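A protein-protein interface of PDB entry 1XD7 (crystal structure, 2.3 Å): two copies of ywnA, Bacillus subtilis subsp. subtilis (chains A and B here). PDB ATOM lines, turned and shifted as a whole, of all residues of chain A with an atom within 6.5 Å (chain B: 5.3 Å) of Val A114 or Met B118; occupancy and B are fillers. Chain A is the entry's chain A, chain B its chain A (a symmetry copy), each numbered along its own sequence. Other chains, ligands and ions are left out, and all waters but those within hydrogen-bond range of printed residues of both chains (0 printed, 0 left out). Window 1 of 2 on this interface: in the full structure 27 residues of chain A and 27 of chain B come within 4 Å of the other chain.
The side-chain hydroxyl (OG) of Ser A113 is in hydrogen-bond range of the side-chain carboxylate (OE1) of Glu B121, at 2.7 Å.
Among the printed residues, pairs that only touch across the chains: Val A114 with Met B118 (3.6 Å), Val A114 with Glu B121 (3.6 Å), Val A114 with Leu B122 (3.9 Å), Ala A117 with Glu B121 (3.9 Å) and Met A118 with Val B114 (3.6 Å).
Of chain B, only Met B118 (3.6 Å), Glu B121 (3.6 Å) and Leu B122 (3.9 Å) come within 4 Å of Val A114. Printed residues of chain A within 4 Å of Glu B121: Ser A113 (2.7 Å), Val A114 (3.6 Å) and Ala A117 (3.9 Å). Printed residues of chain A within 4 Å of Val B114: Met A118. Of the printed residues of chain B, Ala A117 touches Glu B121 (3.9 Å). Printed residues of chain B within 4 Å of Ser A113: Glu B121. The nearest printed residue of chain B that does not touch Val A114 is Glu B119 (6.0 Å).
Along chain B the printed residues that touch a printed residue of chain A span positions 114 to 122. Of the 11 printed residues of chain A, 4 touch a printed residue of chain B. Printed residues of chain A that touch a printed residue of chain B: Ser A113, Val A114, Ala A117 and Met A118. Hydrophobic or aromatic side chains of chain A that line the printed part of chain B: Val A114, Ala A117 and Met A118. Among the printed residues, 6 pairs touch across the chains. Among the printed residues, no Asp or Glu carboxylate lies within 4 Å of a Lys or Arg side-chain nitrogen of the other chain.
Val A114 touches Met B118, and with the chains exchanged Met A118 touches Val B114. Of the 6 pairs that touch across the chains among the printed residues, 2 have their exchanged pair printed and touching as well.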
ATOM      1  N   GLU A 109      28.559  14.860  -3.025  1.00  0.00           N
ATOM      2  CA  GLU A 109      29.462  15.524  -3.934  1.00  0.00           C
ATOM      3  C   GLU A 109      28.753  16.512  -4.859  1.00  0.00           C
ATOM      4  O   GLU A 109      29.278  17.598  -5.129  1.00  0.00           O
ATOM      5  CB  GLU A 109      30.258  14.475  -4.720  1.00  0.00           C
ATOM      6  CG  GLU A 109      29.398  13.496  -5.464  1.00  0.00           C
ATOM      7  CD  GLU A 109      28.687  14.162  -6.620  1.00  0.00           C
ATOM      8  OE1 GLU A 109      27.575  13.719  -6.988  1.00  0.00           O
ATOM      9  OE2 GLU A 109      29.249  15.137  -7.164  1.00  0.00           O
ATOM     10  N   THR A 110      27.559  16.158  -5.334  1.00  0.00           N
ATOM     11  CA  THR A 110      26.831  17.055  -6.231  1.00  0.00           C
ATOM     12  C   THR A 110      26.639  18.394  -5.534  1.00  0.00           C
ATOM     13  O   THR A 110      26.958  19.445  -6.081  1.00  0.00           O
ATOM     14  CB  THR A 110      25.467  16.486  -6.608  1.00  0.00           C
ATOM     15  OG1 THR A 110      25.616  15.127  -7.043  1.00  0.00           O
ATOM     16  CG2 THR A 110      24.867  17.291  -7.735  1.00  0.00           C
ATOM     17  N   PHE A 111      26.129  18.339  -4.309  1.00  0.00           N
ATOM     18  CA  PHE A 111      25.918  19.534  -3.507  1.00  0.00           C
ATOM     19  C   PHE A 111      27.200  20.335  -3.374  1.00  0.00           C
ATOM     20  O   PHE A 111      27.167  21.503  -2.974  1.00  0.00           O
ATOM     21  CB  PHE A 111      25.443  19.165  -2.106  1.00  0.00           C
ATOM     22  CG  PHE A 111      24.084  18.554  -2.072  1.00  0.00           C
ATOM     23  CD1 PHE A 111      23.536  18.131  -0.869  1.00  0.00           C
ATOM     24  CD2 PHE A 111      23.349  18.389  -3.249  1.00  0.00           C
ATOM     25  CE1 PHE A 111      22.278  17.550  -0.833  1.00  0.00           C
ATOM     26  CE2 PHE A 111      22.093  17.810  -3.228  1.00  0.00           C
ATOM     27  CZ  PHE A 111      21.552  17.388  -2.021  1.00  0.00           C
ATOM     28  N   GLU A 112      28.328  19.704  -3.686  1.00  0.00           N
ATOM     29  CA  GLU A 112      29.608  20.384  -3.597  1.00  0.00           C
ATOM     30  C   GLU A 112      29.875  21.064  -4.925  1.00  0.00           C
ATOM     31  O   GLU A 112      30.573  22.066  -4.990  1.00  0.00           O
ATOM     32  CB  GLU A 112      30.719  19.391  -3.276  1.00  0.00           C
ATOM     33  CG  GLU A 112      31.929  20.030  -2.627  1.00  0.00           C
ATOM     34  CD  GLU A 112      32.733  19.029  -1.822  1.00  0.00           C
ATOM     35  OE1 GLU A 112      32.134  18.364  -0.943  1.00  0.00           O
ATOM     36  OE2 GLU A 112      33.956  18.903  -2.063  1.00  0.00           O
ATOM     37  N   SER A 113      29.310  20.510  -5.987  1.00  0.00           N
ATOM     38  CA  SER A 113      29.469  21.084  -7.309  1.00  0.00           C
ATOM     39  C   SER A 113      28.624  22.358  -7.347  1.00  0.00           C
ATOM     40  O   SER A 113      29.087  23.424  -7.761  1.00  0.00           O
ATOM     41  CB  SER A 113      28.982  20.091  -8.365  1.00  0.00           C
ATOM     42  OG  SER A 113      28.965  20.681  -9.652  1.00  0.00           O
ATOM     43  N   VAL A 114      27.378  22.236  -6.903  1.00  0.00           N
ATOM     44  CA  VAL A 114      26.463  23.367  -6.866  1.00  0.00           C
ATOM     45  C   VAL A 114      27.002  24.411  -5.916  1.00  0.00           C
ATOM     46  O   VAL A 114      26.923  25.615  -6.165  1.00  0.00           O
ATOM     47  CB  VAL A 114      25.076  22.935  -6.373  1.00  0.00           C
ATOM     48  CG1 VAL A 114      24.276  24.155  -5.933  1.00  0.00           C
ATOM     49  CG2 VAL A 114      24.357  22.179  -7.477  1.00  0.00           C
ATOM     50  N   GLN A 115      27.544  23.926  -4.813  1.00  0.00           N
ATOM     51  CA  GLN A 115      28.111  24.785  -3.802  1.00  0.00           C
ATOM     52  C   GLN A 115      29.218  25.626  -4.422  1.00  0.00           C
ATOM     53  O   GLN A 115      29.228  26.848  -4.292  1.00  0.00           O
ATOM     54  CB  GLN A 115      28.680  23.926  -2.681  1.00  0.00           C
ATOM     55  CG  GLN A 115      29.432  24.675  -1.598  1.00  0.00           C
ATOM     56  CD  GLN A 115      28.527  25.524  -0.738  1.00  0.00           C
ATOM     57  OE1 GLN A 115      27.383  25.151  -0.459  1.00  0.00           O
ATOM     58  NE2 GLN A 115      29.038  26.666  -0.295  1.00  0.00           N
ATOM     59  N   ARG A 116      30.156  24.963  -5.089  1.00  0.00           N
ATOM     60  CA  ARG A 116      31.271  25.665  -5.708  1.00  0.00           C
ATOM     61  C   ARG A 116      30.708  26.694  -6.679  1.00  0.00           C
ATOM     62  O   ARG A 116      31.191  27.818  -6.746  1.00  0.00           O
ATOM     63  CB  ARG A 116      32.194  24.680  -6.443  1.00  0.00           C
ATOM     64  CG  ARG A 116      32.995  23.721  -5.547  1.00  0.00           C
ATOM     65  CD  ARG A 116      34.069  24.440  -4.747  1.00  0.00           C
ATOM     66  NE  ARG A 116      33.559  24.943  -3.475  1.00  0.00           N
ATOM     67  CZ  ARG A 116      33.349  24.185  -2.399  1.00  0.00           C
ATOM     68  NH1 ARG A 116      33.610  22.883  -2.434  1.00  0.00           N
ATOM     69  NH2 ARG A 116      32.866  24.726  -1.289  1.00  0.00           N
ATOM     70  N   ALA A 117      29.678  26.308  -7.419  1.00  0.00           N
ATOM     71  CA  ALA A 117      29.057  27.225  -8.356  1.00  0.00           C
ATOM     72  C   ALA A 117      28.595  28.461  -7.576  1.00  0.00           C
ATOM     73  O   ALA A 117      29.058  29.565  -7.833  1.00  0.00           O
ATOM     74  CB  ALA A 117      27.894  26.560  -9.036  1.00  0.00           C
ATOM     75  N   MET A 118      27.689  28.267  -6.622  1.00  0.00           N
ATOM     76  CA  MET A 118      27.208  29.365  -5.789  1.00  0.00           C
ATOM     77  C   MET A 118      28.448  30.207  -5.451  1.00  0.00           C
ATOM     78  O   MET A 118      28.545  31.378  -5.830  1.00  0.00           O
ATOM     79  CB  MET A 118      26.568  28.800  -4.499  1.00  0.00           C
ATOM     80  CG  MET A 118      25.674  29.762  -3.673  1.00  0.00           C
ATOM     81  SD  MET A 118      26.207  30.048  -1.932  1.00  0.00           S
ATOM     82  CE  MET A 118      25.624  28.514  -1.131  1.00  0.00           C
ATOM     83  N   GLU A 119      29.413  29.584  -4.782  1.00  0.00           N
ATOM     84  CA  GLU A 119      30.633  30.266  -4.368  1.00  0.00           C
ATOM     85  C   GLU A 119      31.415  30.950  -5.472  1.00  0.00           C
ATOM     86  O   GLU A 119      32.138  31.917  -5.223  1.00  0.00           O
ATOM     87  CB  GLU A 119      31.577  29.302  -3.665  1.00  0.00           C
ATOM     88  CG  GLU A 119      31.120  28.824  -2.310  1.00  0.00           C
ATOM     89  CD  GLU A 119      32.221  28.073  -1.585  1.00  0.00           C
ATOM     90  OE1 GLU A 119      32.757  27.108  -2.167  1.00  0.00           O
ATOM     91  OE2 GLU A 119      32.561  28.445  -0.440  1.00  0.00           O
ATOM     92  N   TYR B  77      14.166  19.554  -8.234  1.00  0.00           N
ATOM     93  CA  TYR B  77      14.153  20.689  -7.331  1.00  0.00           C
ATOM     94  C   TYR B  77      12.839  21.466  -7.346  1.00  0.00           C
ATOM     95  O   TYR B  77      12.173  21.582  -6.325  1.00  0.00           O
ATOM     96  CB  TYR B  77      15.292  21.632  -7.692  1.00  0.00           C
ATOM     97  CG  TYR B  77      15.374  22.866  -6.819  1.00  0.00           C
ATOM     98  CD1 TYR B  77      15.757  22.779  -5.480  1.00  0.00           C
ATOM     99  CD2 TYR B  77      15.101  24.132  -7.344  1.00  0.00           C
ATOM    100  CE1 TYR B  77      15.875  23.928  -4.685  1.00  0.00           C
ATOM    101  CE2 TYR B  77      15.215  25.287  -6.559  1.00  0.00           C
ATOM    102  CZ  TYR B  77      15.604  25.180  -5.233  1.00  0.00           C
ATOM    103  OH  TYR B  77      15.744  26.324  -4.468  1.00  0.00           O
ATOM    104  N   SER B 113      21.658  36.122  -9.883  1.00  0.00           N
ATOM    105  CA  SER B 113      22.768  35.641 -10.682  1.00  0.00           C
ATOM    106  C   SER B 113      23.250  34.340 -10.038  1.00  0.00           C
ATOM    107  O   SER B 113      23.436  33.322 -10.709  1.00  0.00           O
ATOM    108  CB  SER B 113      23.889  36.680 -10.687  1.00  0.00           C
ATOM    109  OG  SER B 113      25.053  36.174 -11.316  1.00  0.00           O
ATOM    110  N   VAL B 114      23.445  34.385  -8.726  1.00  0.00           N
ATOM    111  CA  VAL B 114      23.889  33.220  -7.975  1.00  0.00           C
ATOM    112  C   VAL B 114      22.838  32.139  -8.070  1.00  0.00           C
ATOM    113  O   VAL B 114      23.141  30.951  -8.195  1.00  0.00           O
ATOM    114  CB  VAL B 114      24.096  33.566  -6.495  1.00  0.00           C
ATOM    115  CG1 VAL B 114      24.134  32.290  -5.662  1.00  0.00           C
ATOM    116  CG2 VAL B 114      25.379  34.363  -6.333  1.00  0.00           C
ATOM    117  N   GLN B 115      21.593  32.572  -7.996  1.00  0.00           N
ATOM    118  CA  GLN B 115      20.467  31.673  -8.074  1.00  0.00           C
ATOM    119  C   GLN B 115      20.521  30.917  -9.394  1.00  0.00           C
ATOM    120  O   GLN B 115      20.449  29.690  -9.421  1.00  0.00           O
ATOM    121  CB  GLN B 115      19.178  32.479  -7.993  1.00  0.00           C
ATOM    122  CG  GLN B 115      17.898  31.692  -8.193  1.00  0.00           C
ATOM    123  CD  GLN B 115      17.603  30.755  -7.046  1.00  0.00           C
ATOM    124  OE1 GLN B 115      17.885  31.065  -5.884  1.00  0.00           O
ATOM    125  NE2 GLN B 115      17.015  29.607  -7.361  1.00  0.00           N
ATOM    126  N   ARG B 116      20.638  31.657 -10.492  1.00  0.00           N
ATOM    127  CA  ARG B 116      20.682  31.040 -11.809  1.00  0.00           C
ATOM    128  C   ARG B 116      21.842  30.054 -11.837  1.00  0.00           C
ATOM    129  O   ARG B 116      21.717  28.956 -12.366  1.00  0.00           O
ATOM    130  CB  ARG B 116      20.854  32.105 -12.904  1.00  0.00           C
ATOM    131  CG  ARG B 116      19.650  33.034 -13.126  1.00  0.00           C
ATOM    132  CD  ARG B 116      18.465  32.306 -13.740  1.00  0.00           C
ATOM    133  NE  ARG B 116      17.606  31.703 -12.725  1.00  0.00           N
ATOM    134  CZ  ARG B 116      16.730  32.382 -11.985  1.00  0.00           C
ATOM    135  NH1 ARG B 116      16.586  33.693 -12.147  1.00  0.00           N
ATOM    136  NH2 ARG B 116      16.003  31.753 -11.072  1.00  0.00           N
ATOM    137  N   ALA B 117      22.967  30.447 -11.254  1.00  0.00           N
ATOM    138  CA  ALA B 117      24.120  29.569 -11.207  1.00  0.00           C
ATOM    139  C   ALA B 117      23.700  28.269 -10.513  1.00  0.00           C
ATOM    140  O   ALA B 117      23.749  27.201 -11.113  1.00  0.00           O
ATOM    141  CB  ALA B 117      25.244  30.231 -10.462  1.00  0.00           C
ATOM    142  N   MET B 118      23.282  28.365  -9.254  1.00  0.00           N
ATOM    143  CA  MET B 118      22.820  27.199  -8.510  1.00  0.00           C
ATOM    144  C   MET B 118      21.967  26.385  -9.495  1.00  0.00           C
ATOM    145  O   MET B 118      22.300  25.245  -9.835  1.00  0.00           O
ATOM    146  CB  MET B 118      21.966  27.655  -7.303  1.00  0.00           C
ATOM    147  CG  MET B 118      21.699  26.608  -6.189  1.00  0.00           C
ATOM    148  SD  MET B 118      19.926  26.231  -5.857  1.00  0.00           S
ATOM    149  CE  MET B 118      19.438  27.687  -4.869  1.00  0.00           C
ATOM    150  N   GLU B 119      20.898  27.000  -9.990  1.00  0.00           N
ATOM    151  CA  GLU B 119      19.982  26.341 -10.913  1.00  0.00           C
ATOM    152  C   GLU B 119      20.610  25.759 -12.165  1.00  0.00           C
ATOM    153  O   GLU B 119      20.085  24.807 -12.745  1.00  0.00           O
ATOM    154  CB  GLU B 119      18.879  27.293 -11.350  1.00  0.00           C
ATOM    155  CG  GLU B 119      17.885  27.664 -10.280  1.00  0.00           C
ATOM    156  CD  GLU B 119      16.696  28.409 -10.859  1.00  0.00           C
ATOM    157  OE1 GLU B 119      16.918  29.430 -11.543  1.00  0.00           O
ATOM    158  OE2 GLU B 119      15.543  27.978 -10.644  1.00  0.00           O
ATOM    159  N   ASN B 120      21.718  26.331 -12.608  1.00  0.00           N
ATOM    160  CA  ASN B 120      22.337  25.818 -13.818  1.00  0.00           C
ATOM    161  C   ASN B 120      23.094  24.503 -13.618  1.00  0.00           C
ATOM    162  O   ASN B 120      23.149  23.676 -14.528  1.00  0.00           O
ATOM    163  CB  ASN B 120      23.202  26.902 -14.452  1.00  0.00           C
ATOM    164  CG  ASN B 120      22.374  27.881 -15.271  1.00  0.00           C
ATOM    165  OD1 ASN B 120      22.850  28.947 -15.656  1.00  0.00           O
ATOM    166  ND2 ASN B 120      21.126  27.515 -15.547  1.00  0.00           N
ATOM    167  N   GLU B 121      23.660  24.294 -12.438  1.00  0.00           N
ATOM    168  CA  GLU B 121      24.327  23.031 -12.166  1.00  0.00           C
ATOM    169  C   GLU B 121      23.248  21.955 -12.078  1.00  0.00           C
ATOM    170  O   GLU B 121      23.289  20.958 -12.796  1.00  0.00           O
ATOM    171  CB  GLU B 121      25.086  23.088 -10.845  1.00  0.00           C
ATOM    172  CG  GLU B 121      26.513  23.521 -11.015  1.00  0.00           C
ATOM    173  CD  GLU B 121      27.232  22.660 -12.028  1.00  0.00           C
ATOM    174  OE1 GLU B 121      27.397  21.453 -11.755  1.00  0.00           O
ATOM    175  OE2 GLU B 121      27.621  23.180 -13.097  1.00  0.00           O
ATOM    176  N   LEU B 122      22.264  22.177 -11.214  1.00  0.00           N
ATOM    177  CA  LEU B 122      21.181  21.218 -11.033  1.00  0.00           C
ATOM    178  C   LEU B 122      20.592  20.741 -12.334  1.00  0.00           C
ATOM    179  O   LEU B 122      19.971  19.686 -12.386  1.00  0.00           O
ATOM    180  CB  LEU B 122      20.056  21.824 -10.211  1.00  0.00           C
ATOM    181  CG  LEU B 122      20.395  22.163  -8.773  1.00  0.00           C
ATOM    182  CD1 LEU B 122      19.212  22.902  -8.180  1.00  0.00           C
ATOM    183  CD2 LEU B 122      20.706  20.901  -7.994  1.00  0.00           C
